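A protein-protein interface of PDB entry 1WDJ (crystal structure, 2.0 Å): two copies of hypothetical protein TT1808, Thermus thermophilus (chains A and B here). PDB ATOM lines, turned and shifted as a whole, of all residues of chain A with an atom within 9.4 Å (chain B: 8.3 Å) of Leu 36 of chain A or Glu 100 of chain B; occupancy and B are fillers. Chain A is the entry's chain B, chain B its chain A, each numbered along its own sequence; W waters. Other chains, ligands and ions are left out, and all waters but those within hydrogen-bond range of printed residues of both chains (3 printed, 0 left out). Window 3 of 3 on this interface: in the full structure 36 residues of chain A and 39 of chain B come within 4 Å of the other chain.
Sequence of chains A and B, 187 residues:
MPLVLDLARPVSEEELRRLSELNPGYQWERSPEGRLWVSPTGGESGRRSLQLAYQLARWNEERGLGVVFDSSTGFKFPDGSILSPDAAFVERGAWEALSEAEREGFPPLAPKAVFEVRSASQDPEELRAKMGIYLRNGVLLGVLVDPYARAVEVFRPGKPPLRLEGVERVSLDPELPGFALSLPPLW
CD2 of Leu 36 of chain A touches OE2 of Glu 100 of chain B, at 3.5 Å. Val 38 of chain A touches Glu 104 of chain B (CG2 to CG, 3.0 Å). CG of Arg 17 of chain B touches OG of Ser 39 of chain A, at 3.8 Å. Gly 42 of chain A touches Glu 104 of chain B. Gly 42 of chain A touches Gly 105 of chain B (CA to O, 3.3 Å). Gly 43 of chain A touches Trp 95 of chain B (CA to CH2, 3.9 Å). Glu 44 of chain A touches Trp 95 of chain B. OE2 of Glu 104 of chain B touches CB of Glu 44 of chain A (3.4 Å). Tyr 148 of chain A touches Glu 104 of chain B.
Printed residues of chain B within 4 Å of Val 38 of chain A: Arg 17 and Glu 104. Printed residues of chain B within 4 Å of Gly 43 of chain A: Trp 95, Arg 103 and Gly 105. Of the printed residues of chain A, Arg 17 of chain B touches Trp 37, Val 38 and Ser 39. No residue of chain A comes within 4 Å of Ser 99 of chain B. Glu 100 of chain B touches just one residue of chain A: Leu 36 (3.5 Å). Ala 101 of chain B touches none of the printed residues of chain A. The nearest residue of chain B that does not touch Leu 36 of chain A is Ala 101 of chain B (4.2 Å).
Water W3 lies within hydrogen-bond range of the side-chain carboxylate of Glu 44 of chain A (2.5 Å), the indole nitrogen of Trp 95 of chain B (2.9 Å) and the guanidinium group of Arg 103 of chain B (3.3 Å). Water W1 lies within hydrogen-bond range of the backbone carbonyl oxygen of Trp 37 of chain A (2.5 Å) and the backbone carbonyl oxygen of Ala 101 of chain B (2.9 Å). Water W2 lies within hydrogen-bond range of OE2 of Glu 104 of chain B (2.7 Å), N of Ser 45 of chain A (2.9 Å), O of Ser 39 of chain A (3.2 Å) and N of Glu 44 of chain A (3.4 Å).
The backbone carbonyl oxygen of Val 38 of chain A lies within hydrogen-bond range of the guanidinium group of Arg 17 of chain B. N of Gly 43 of chain A lies close to O of Arg 103 of chain B (3.0 Å). The backbone carbonyl oxygen (O) of Arg 103 of chain B lies within hydrogen-bond range of the backbone NH (N) of Glu 44 of chain A, 2.8 Å away. O of Glu 104 of chain B is in hydrogen-bond range of N of Ser 39 of chain A (3.4 Å). The backbone carbonyl oxygen of Gly 105 of chain B is in hydrogen-bond range of the backbone NH of Gly 43 of chain A, at 2.9 Å. NE1 of Trp 37 of chain A lies close to NH1 of Arg 17 of chain B (3.2 Å).
No position is printed for both chains.
Of the 12 printed residues of chain B, 6 touch a printed residue of chain A. Hydrophobic or aromatic side chains of chain B that line the printed part of chain A: Trp 95. Hydrophobic or aromatic side chains of chain A that line the printed part of chain B: Leu 36, Trp 37, Val 38 and Tyr 148. Among the printed residues, no Asp or Glu carboxylate lies within 4 Å of a Lys or Arg side-chain nitrogen of the other chain.
OE1 of Glu 96 of chain B is in salt-bridge range of NH1 of Arg 103 of chain B. The backbone carbonyl oxygen (O) of Leu 98 of chain B sits at hydrogen-bond distance from the guanidinium group (NE) of Arg 103 of chain B. The side-chain hydroxyl of Ser 121 of chain A lies close to the backbone carbonyl oxygen of Val 38 of chain A. The backbone carbonyl oxygen of Ser 39 of chain A sits at hydrogen-bond distance from the side-chain hydroxyl of Ser 45 of chain A, 3.3 Å away. The guanidinium group (NH2) of Arg 48 of chain A is in salt-bridge range of the side-chain carboxylate (OE1) of Glu 44 of chain A (3.4 Å). The side-chain hydroxyl (OH) of Tyr 148 of chain A lies within hydrogen-bond range of the guanidinium group (NH1) of Arg 48 of chain A.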
ATOM      1  N   LEU A  36     -18.076  -2.916  -9.160  1.00  0.00           N
ATOM      2  CA  LEU A  36     -18.661  -2.091  -8.111  1.00  0.00           C
ATOM      3  C   LEU A  36     -19.932  -2.684  -7.512  1.00  0.00           C
ATOM      4  O   LEU A  36     -20.597  -3.529  -8.118  1.00  0.00           O
ATOM      5  CB  LEU A  36     -18.945  -0.680  -8.639  1.00  0.00           C
ATOM      6  CG  LEU A  36     -19.551  -0.503 -10.035  1.00  0.00           C
ATOM      7  CD1 LEU A  36     -20.786  -1.360 -10.201  1.00  0.00           C
ATOM      8  CD2 LEU A  36     -19.877   0.965 -10.244  1.00  0.00           C
ATOM      9  N   TRP A  37     -20.256  -2.226  -6.308  1.00  0.00           N
ATOM     10  CA  TRP A  37     -21.430  -2.684  -5.574  1.00  0.00           C
ATOM     11  C   TRP A  37     -22.721  -2.334  -6.314  1.00  0.00           C
ATOM     12  O   TRP A  37     -23.048  -1.163  -6.488  1.00  0.00           O
ATOM     13  CB  TRP A  37     -21.448  -2.040  -4.193  1.00  0.00           C
ATOM     14  CG  TRP A  37     -22.302  -2.771  -3.240  1.00  0.00           C
ATOM     15  CD1 TRP A  37     -21.989  -3.921  -2.576  1.00  0.00           C
ATOM     16  CD2 TRP A  37     -23.636  -2.435  -2.860  1.00  0.00           C
ATOM     17  NE1 TRP A  37     -23.046  -4.326  -1.804  1.00  0.00           N
ATOM     18  CE2 TRP A  37     -24.073  -3.431  -1.958  1.00  0.00           C
ATOM     19  CE3 TRP A  37     -24.507  -1.390  -3.194  1.00  0.00           C
ATOM     20  CZ2 TRP A  37     -25.347  -3.413  -1.381  1.00  0.00           C
ATOM     21  CZ3 TRP A  37     -25.776  -1.371  -2.618  1.00  0.00           C
ATOM     22  CH2 TRP A  37     -26.179  -2.379  -1.720  1.00  0.00           C
ATOM     23  N   VAL A  38     -23.461  -3.355  -6.726  1.00  0.00           N
ATOM     24  CA  VAL A  38     -24.702  -3.140  -7.468  1.00  0.00           C
ATOM     25  C   VAL A  38     -25.906  -3.825  -6.818  1.00  0.00           C
ATOM     26  O   VAL A  38     -25.789  -4.917  -6.258  1.00  0.00           O
ATOM     27  CB  VAL A  38     -24.551  -3.665  -8.935  1.00  0.00           C
ATOM     28  CG1 VAL A  38     -25.860  -3.505  -9.718  1.00  0.00           C
ATOM     29  CG2 VAL A  38     -23.426  -2.920  -9.630  1.00  0.00           C
ATOM     30  N   SER A  39     -27.066  -3.180  -6.896  1.00  0.00           N
ATOM     31  CA  SER A  39     -28.271  -3.773  -6.341  1.00  0.00           C
ATOM     32  C   SER A  39     -29.380  -3.882  -7.385  1.00  0.00           C
ATOM     33  O   SER A  39     -29.585  -2.971  -8.185  1.00  0.00           O
ATOM     34  CB  SER A  39     -28.786  -2.955  -5.154  1.00  0.00           C
ATOM     35  OG  SER A  39     -29.901  -3.597  -4.541  1.00  0.00           O
ATOM     36  N   GLY A  42     -31.589  -1.183  -6.940  1.00  0.00           N
ATOM     37  CA  GLY A  42     -30.918   0.117  -6.965  1.00  0.00           C
ATOM     38  C   GLY A  42     -31.430   1.018  -8.095  1.00  0.00           C
ATOM     39  O   GLY A  42     -32.313   0.624  -8.862  1.00  0.00           O
ATOM     40  N   GLY A  43     -30.865   2.218  -8.215  1.00  0.00           N
ATOM     41  CA  GLY A  43     -31.305   3.160  -9.230  1.00  0.00           C
ATOM     42  C   GLY A  43     -31.225   2.732 -10.691  1.00  0.00           C
ATOM     43  O   GLY A  43     -32.237   2.727 -11.401  1.00  0.00           O
ATOM     44  N   GLU A  44     -30.028   2.388 -11.157  1.00  0.00           N
ATOM     45  CA  GLU A  44     -29.851   1.980 -12.555  1.00  0.00           C
ATOM     46  C   GLU A  44     -30.777   0.844 -12.972  1.00  0.00           C
ATOM     47  O   GLU A  44     -31.406   0.917 -14.030  1.00  0.00           O
ATOM     48  CB  GLU A  44     -28.385   1.594 -12.816  1.00  0.00           C
ATOM     49  CG  GLU A  44     -27.487   2.796 -12.971  1.00  0.00           C
ATOM     50  CD  GLU A  44     -27.759   3.534 -14.263  1.00  0.00           C
ATOM     51  OE1 GLU A  44     -27.305   3.056 -15.322  1.00  0.00           O
ATOM     52  OE2 GLU A  44     -28.440   4.576 -14.228  1.00  0.00           O
ATOM     53  N   SER A  45     -30.867  -0.200 -12.148  1.00  0.00           N
ATOM     54  CA  SER A  45     -31.739  -1.330 -12.469  1.00  0.00           C
ATOM     55  C   SER A  45     -33.188  -0.839 -12.549  1.00  0.00           C
ATOM     56  O   SER A  45     -33.929  -1.221 -13.463  1.00  0.00           O
ATOM     57  CB  SER A  45     -31.635  -2.441 -11.406  1.00  0.00           C
ATOM     58  OG  SER A  45     -30.344  -3.027 -11.368  1.00  0.00           O
ATOM     59  N   ARG A  48     -33.843   1.145 -15.706  1.00  0.00           N
ATOM     60  CA  ARG A  48     -33.943   0.272 -16.875  1.00  0.00           C
ATOM     61  C   ARG A  48     -35.224  -0.557 -16.913  1.00  0.00           C
ATOM     62  O   ARG A  48     -35.891  -0.627 -17.953  1.00  0.00           O
ATOM     63  CB  ARG A  48     -32.732  -0.659 -16.963  1.00  0.00           C
ATOM     64  CG  ARG A  48     -31.445   0.071 -17.229  1.00  0.00           C
ATOM     65  CD  ARG A  48     -30.485  -0.805 -18.002  1.00  0.00           C
ATOM     66  NE  ARG A  48     -29.241  -0.097 -18.279  1.00  0.00           N
ATOM     67  CZ  ARG A  48     -28.256   0.026 -17.400  1.00  0.00           C
ATOM     68  NH1 ARG A  48     -28.381  -0.523 -16.195  1.00  0.00           N
ATOM     69  NH2 ARG A  48     -27.159   0.697 -17.723  1.00  0.00           N
ATOM     70  N   SER A 119     -28.696  -6.770 -14.412  1.00  0.00           N
ATOM     71  CA  SER A 119     -28.065  -5.656 -13.719  1.00  0.00           C
ATOM     72  C   SER A 119     -26.668  -6.174 -13.394  1.00  0.00           C
ATOM     73  O   SER A 119     -26.488  -7.376 -13.154  1.00  0.00           O
ATOM     74  CB  SER A 119     -28.851  -5.268 -12.450  1.00  0.00           C
ATOM     75  OG  SER A 119     -28.844  -6.293 -11.483  1.00  0.00           O
ATOM     76  N   ALA A 120     -25.690  -5.272 -13.438  1.00  0.00           N
ATOM     77  CA  ALA A 120     -24.281  -5.588 -13.183  1.00  0.00           C
ATOM     78  C   ALA A 120     -24.052  -6.638 -12.088  1.00  0.00           C
ATOM     79  O   ALA A 120     -23.121  -7.443 -12.170  1.00  0.00           O
ATOM     80  CB  ALA A 120     -23.535  -4.309 -12.848  1.00  0.00           C
ATOM     81  N   SER A 121     -24.920  -6.621 -11.078  1.00  0.00           N
ATOM     82  CA  SER A 121     -24.871  -7.536  -9.941  1.00  0.00           C
ATOM     83  C   SER A 121     -25.192  -9.000 -10.291  1.00  0.00           C
ATOM     84  O   SER A 121     -25.123  -9.877  -9.421  1.00  0.00           O
ATOM     85  CB  SER A 121     -25.846  -7.038  -8.864  1.00  0.00           C
ATOM     86  OG  SER A 121     -25.991  -7.967  -7.804  1.00  0.00           O
ATOM     87  N   GLN A 122     -25.532  -9.267 -11.552  1.00  0.00           N
ATOM     88  CA  GLN A 122     -25.877 -10.627 -11.982  1.00  0.00           C
ATOM     89  C   GLN A 122     -25.027 -11.147 -13.142  1.00  0.00           C
ATOM     90  O   GLN A 122     -24.732 -10.409 -14.083  1.00  0.00           O
ATOM     91  CB  GLN A 122     -27.353 -10.681 -12.390  1.00  0.00           C
ATOM     92  CG  GLN A 122     -28.305 -10.137 -11.346  1.00  0.00           C
ATOM     93  CD  GLN A 122     -29.723 -10.020 -11.866  1.00  0.00           C
ATOM     94  OE1 GLN A 122     -29.963  -9.408 -12.911  1.00  0.00           O
ATOM     95  NE2 GLN A 122     -30.676 -10.597 -11.138  1.00  0.00           N
ATOM     96  N   TYR A 148     -25.453  -4.229 -20.625  1.00  0.00           N
ATOM     97  CA  TYR A 148     -24.006  -4.134 -20.702  1.00  0.00           C
ATOM     98  C   TYR A 148     -23.497  -4.701 -22.031  1.00  0.00           C
ATOM     99  O   TYR A 148     -22.809  -4.007 -22.773  1.00  0.00           O
ATOM    100  CB  TYR A 148     -23.391  -4.809 -19.467  1.00  0.00           C
ATOM    101  CG  TYR A 148     -24.006  -4.232 -18.199  1.00  0.00           C
ATOM    102  CD1 TYR A 148     -25.044  -4.891 -17.540  1.00  0.00           C
ATOM    103  CD2 TYR A 148     -23.637  -2.961 -17.733  1.00  0.00           C
ATOM    104  CE1 TYR A 148     -25.705  -4.302 -16.463  1.00  0.00           C
ATOM    105  CE2 TYR A 148     -24.288  -2.366 -16.659  1.00  0.00           C
ATOM    106  CZ  TYR A 148     -25.323  -3.041 -16.028  1.00  0.00           C
ATOM    107  OH  TYR A 148     -25.985  -2.461 -14.965  1.00  0.00           O
ATOM    108  N   ARG B  17     -30.180  -5.597   0.177  1.00  0.00           N
ATOM    109  CA  ARG B  17     -29.984  -6.194  -1.140  1.00  0.00           C
ATOM    110  C   ARG B  17     -30.147  -7.702  -1.076  1.00  0.00           C
ATOM    111  O   ARG B  17     -30.839  -8.311  -1.890  1.00  0.00           O
ATOM    112  CB  ARG B  17     -28.579  -5.886  -1.696  1.00  0.00           C
ATOM    113  CG  ARG B  17     -28.309  -6.636  -3.015  1.00  0.00           C
ATOM    114  CD  ARG B  17     -26.936  -6.356  -3.630  1.00  0.00           C
ATOM    115  NE  ARG B  17     -25.857  -7.113  -3.002  1.00  0.00           N
ATOM    116  CZ  ARG B  17     -24.572  -6.967  -3.316  1.00  0.00           C
ATOM    117  NH1 ARG B  17     -24.220  -6.095  -4.250  1.00  0.00           N
ATOM    118  NH2 ARG B  17     -23.631  -7.678  -2.699  1.00  0.00           N
ATOM    119  N   TRP B  95     -29.918  13.697 -10.649  1.00  0.00           N
ATOM    120  CA  TRP B  95     -29.499  12.343 -10.982  1.00  0.00           C
ATOM    121  C   TRP B  95     -28.059  12.277 -11.488  1.00  0.00           C
ATOM    122  O   TRP B  95     -27.270  11.402 -11.081  1.00  0.00           O
ATOM    123  CB  TRP B  95     -30.438  11.766 -12.046  1.00  0.00           C
ATOM    124  CG  TRP B  95     -30.108  10.374 -12.451  1.00  0.00           C
ATOM    125  CD1 TRP B  95     -29.689   9.962 -13.675  1.00  0.00           C
ATOM    126  CD2 TRP B  95     -30.183   9.199 -11.630  1.00  0.00           C
ATOM    127  NE1 TRP B  95     -29.497   8.597 -13.674  1.00  0.00           N
ATOM    128  CE2 TRP B  95     -29.793   8.108 -12.432  1.00  0.00           C
ATOM    129  CE3 TRP B  95     -30.541   8.967 -10.295  1.00  0.00           C
ATOM    130  CZ2 TRP B  95     -29.751   6.803 -11.948  1.00  0.00           C
ATOM    131  CZ3 TRP B  95     -30.498   7.661  -9.809  1.00  0.00           C
ATOM    132  CH2 TRP B  95     -30.105   6.597 -10.634  1.00  0.00           C
ATOM    133  N   GLU B  96     -27.733  13.205 -12.387  1.00  0.00           N
ATOM    134  CA  GLU B  96     -26.409  13.269 -12.981  1.00  0.00           C
ATOM    135  C   GLU B  96     -25.327  13.549 -11.938  1.00  0.00           C
ATOM    136  O   GLU B  96     -24.219  13.033 -12.039  1.00  0.00           O
ATOM    137  CB  GLU B  96     -26.373  14.330 -14.085  1.00  0.00           C
ATOM    138  CG  GLU B  96     -27.264  14.018 -15.301  1.00  0.00           C
ATOM    139  CD  GLU B  96     -27.130  12.577 -15.792  1.00  0.00           C
ATOM    140  OE1 GLU B  96     -26.010  12.017 -15.748  1.00  0.00           O
ATOM    141  OE2 GLU B  96     -28.149  12.003 -16.239  1.00  0.00           O
ATOM    142  N   ALA B  97     -25.655  14.354 -10.934  1.00  0.00           N
ATOM    143  CA  ALA B  97     -24.712  14.677  -9.872  1.00  0.00           C
ATOM    144  C   ALA B  97     -24.187  13.426  -9.129  1.00  0.00           C
ATOM    145  O   ALA B  97     -23.149  13.470  -8.448  1.00  0.00           O
ATOM    146  CB  ALA B  97     -25.374  15.623  -8.891  1.00  0.00           C
ATOM    147  N   LEU B  98     -24.897  12.312  -9.250  1.00  0.00           N
ATOM    148  CA  LEU B  98     -24.483  11.095  -8.572  1.00  0.00           C
ATOM    149  C   LEU B  98     -23.400  10.313  -9.320  1.00  0.00           C
ATOM    150  O   LEU B  98     -23.337  10.317 -10.563  1.00  0.00           O
ATOM    151  CB  LEU B  98     -25.680  10.172  -8.354  1.00  0.00           C
ATOM    152  CG  LEU B  98     -26.873  10.662  -7.542  1.00  0.00           C
ATOM    153  CD1 LEU B  98     -27.913   9.554  -7.556  1.00  0.00           C
ATOM    154  CD2 LEU B  98     -26.462  11.025  -6.107  1.00  0.00           C
ATOM    155  N   SER B  99     -22.568   9.621  -8.543  1.00  0.00           N
ATOM    156  CA  SER B  99     -21.494   8.809  -9.091  1.00  0.00           C
ATOM    157  C   SER B  99     -22.125   7.539  -9.631  1.00  0.00           C
ATOM    158  O   SER B  99     -23.251   7.191  -9.285  1.00  0.00           O
ATOM    159  CB  SER B  99     -20.468   8.455  -8.005  1.00  0.00           C
ATOM    160  OG  SER B  99     -20.932   7.410  -7.161  1.00  0.00           O
ATOM    161  N   GLU B 100     -21.396   6.848 -10.487  1.00  0.00           N
ATOM    162  CA  GLU B 100     -21.893   5.629 -11.078  1.00  0.00           C
ATOM    163  C   GLU B 100     -22.293   4.647  -9.980  1.00  0.00           C
ATOM    164  O   GLU B 100     -23.267   3.916 -10.115  1.00  0.00           O
ATOM    165  CB  GLU B 100     -20.807   5.032 -11.963  1.00  0.00           C
ATOM    166  CG  GLU B 100     -21.252   3.879 -12.817  1.00  0.00           C
ATOM    167  CD  GLU B 100     -20.074   3.186 -13.479  1.00  0.00           C
ATOM    168  OE1 GLU B 100     -19.125   3.896 -13.891  1.00  0.00           O
ATOM    169  OE2 GLU B 100     -20.099   1.939 -13.593  1.00  0.00           O
ATOM    170  N   ALA B 101     -21.539   4.642  -8.886  1.00  0.00           N
ATOM    171  CA  ALA B 101     -21.806   3.748  -7.762  1.00  0.00           C
ATOM    172  C   ALA B 101     -23.086   4.142  -7.023  1.00  0.00           C
ATOM    173  O   ALA B 101     -23.867   3.283  -6.583  1.00  0.00           O
ATOM    174  CB  ALA B 101     -20.624   3.767  -6.793  1.00  0.00           C
ATOM    175  N   GLU B 102     -23.291   5.444  -6.882  1.00  0.00           N
ATOM    176  CA  GLU B 102     -24.464   5.943  -6.184  1.00  0.00           C
ATOM    177  C   GLU B 102     -25.753   5.653  -6.953  1.00  0.00           C
ATOM    178  O   GLU B 102     -26.803   5.412  -6.346  1.00  0.00           O
ATOM    179  CB  GLU B 102     -24.325   7.450  -5.937  1.00  0.00           C
ATOM    180  CG  GLU B 102     -23.114   7.812  -5.099  1.00  0.00           C
ATOM    181  CD  GLU B 102     -22.977   9.305  -4.889  1.00  0.00           C
ATOM    182  OE1 GLU B 102     -23.017  10.058  -5.879  1.00  0.00           O
ATOM    183  OE2 GLU B 102     -22.826   9.730  -3.733  1.00  0.00           O
ATOM    184  N   ARG B 103     -25.671   5.675  -8.279  1.00  0.00           N
ATOM    185  CA  ARG B 103     -26.831   5.414  -9.125  1.00  0.00           C
ATOM    186  C   ARG B 103     -27.142   3.937  -9.141  1.00  0.00           C
ATOM    187  O   ARG B 103     -28.304   3.530  -9.223  1.00  0.00           O
ATOM    188  CB  ARG B 103     -26.547   5.850 -10.557  1.00  0.00           C
ATOM    189  CG  ARG B 103     -26.048   7.275 -10.685  1.00  0.00           C
ATOM    190  CD  ARG B 103     -25.707   7.615 -12.132  1.00  0.00           C
ATOM    191  NE  ARG B 103     -25.003   8.888 -12.186  1.00  0.00           N
ATOM    192  CZ  ARG B 103     -24.876   9.643 -13.270  1.00  0.00           C
ATOM    193  NH1 ARG B 103     -25.411   9.259 -14.429  1.00  0.00           N
ATOM    194  NH2 ARG B 103     -24.230  10.800 -13.185  1.00  0.00           N
ATOM    195  N   GLU B 104     -26.085   3.130  -9.069  1.00  0.00           N
ATOM    196  CA  GLU B 104     -26.214   1.683  -9.121  1.00  0.00           C
ATOM    197  C   GLU B 104     -26.750   1.098  -7.811  1.00  0.00           C
ATOM    198  O   GLU B 104     -27.424   0.062  -7.817  1.00  0.00           O
ATOM    199  CB  GLU B 104     -24.858   1.074  -9.494  1.00  0.00           C
ATOM    200  CG  GLU B 104     -24.927  -0.317 -10.060  1.00  0.00           C
ATOM    201  CD  GLU B 104     -25.532  -0.372 -11.452  1.00  0.00           C
ATOM    202  OE1 GLU B 104     -24.967   0.269 -12.359  1.00  0.00           O
ATOM    203  OE2 GLU B 104     -26.565  -1.060 -11.641  1.00  0.00           O
ATOM    204  N   GLY B 105     -26.452   1.757  -6.692  1.00  0.00           N
ATOM    205  CA  GLY B 105     -26.956   1.291  -5.411  1.00  0.00           C
ATOM    206  C   GLY B 105     -28.232   2.071  -5.127  1.00  0.00           C
ATOM    207  O   GLY B 105     -28.898   2.509  -6.074  1.00  0.00           O
HETATM  208  O   HOH W   1     -22.904   0.970  -5.155  1.00  0.00           O
HETATM  209  O   HOH W   2     -28.751  -0.651 -10.180  1.00  0.00           O
HETATM  210  O   HOH W   3     -27.565   6.804 -14.938  1.00  0.00           O
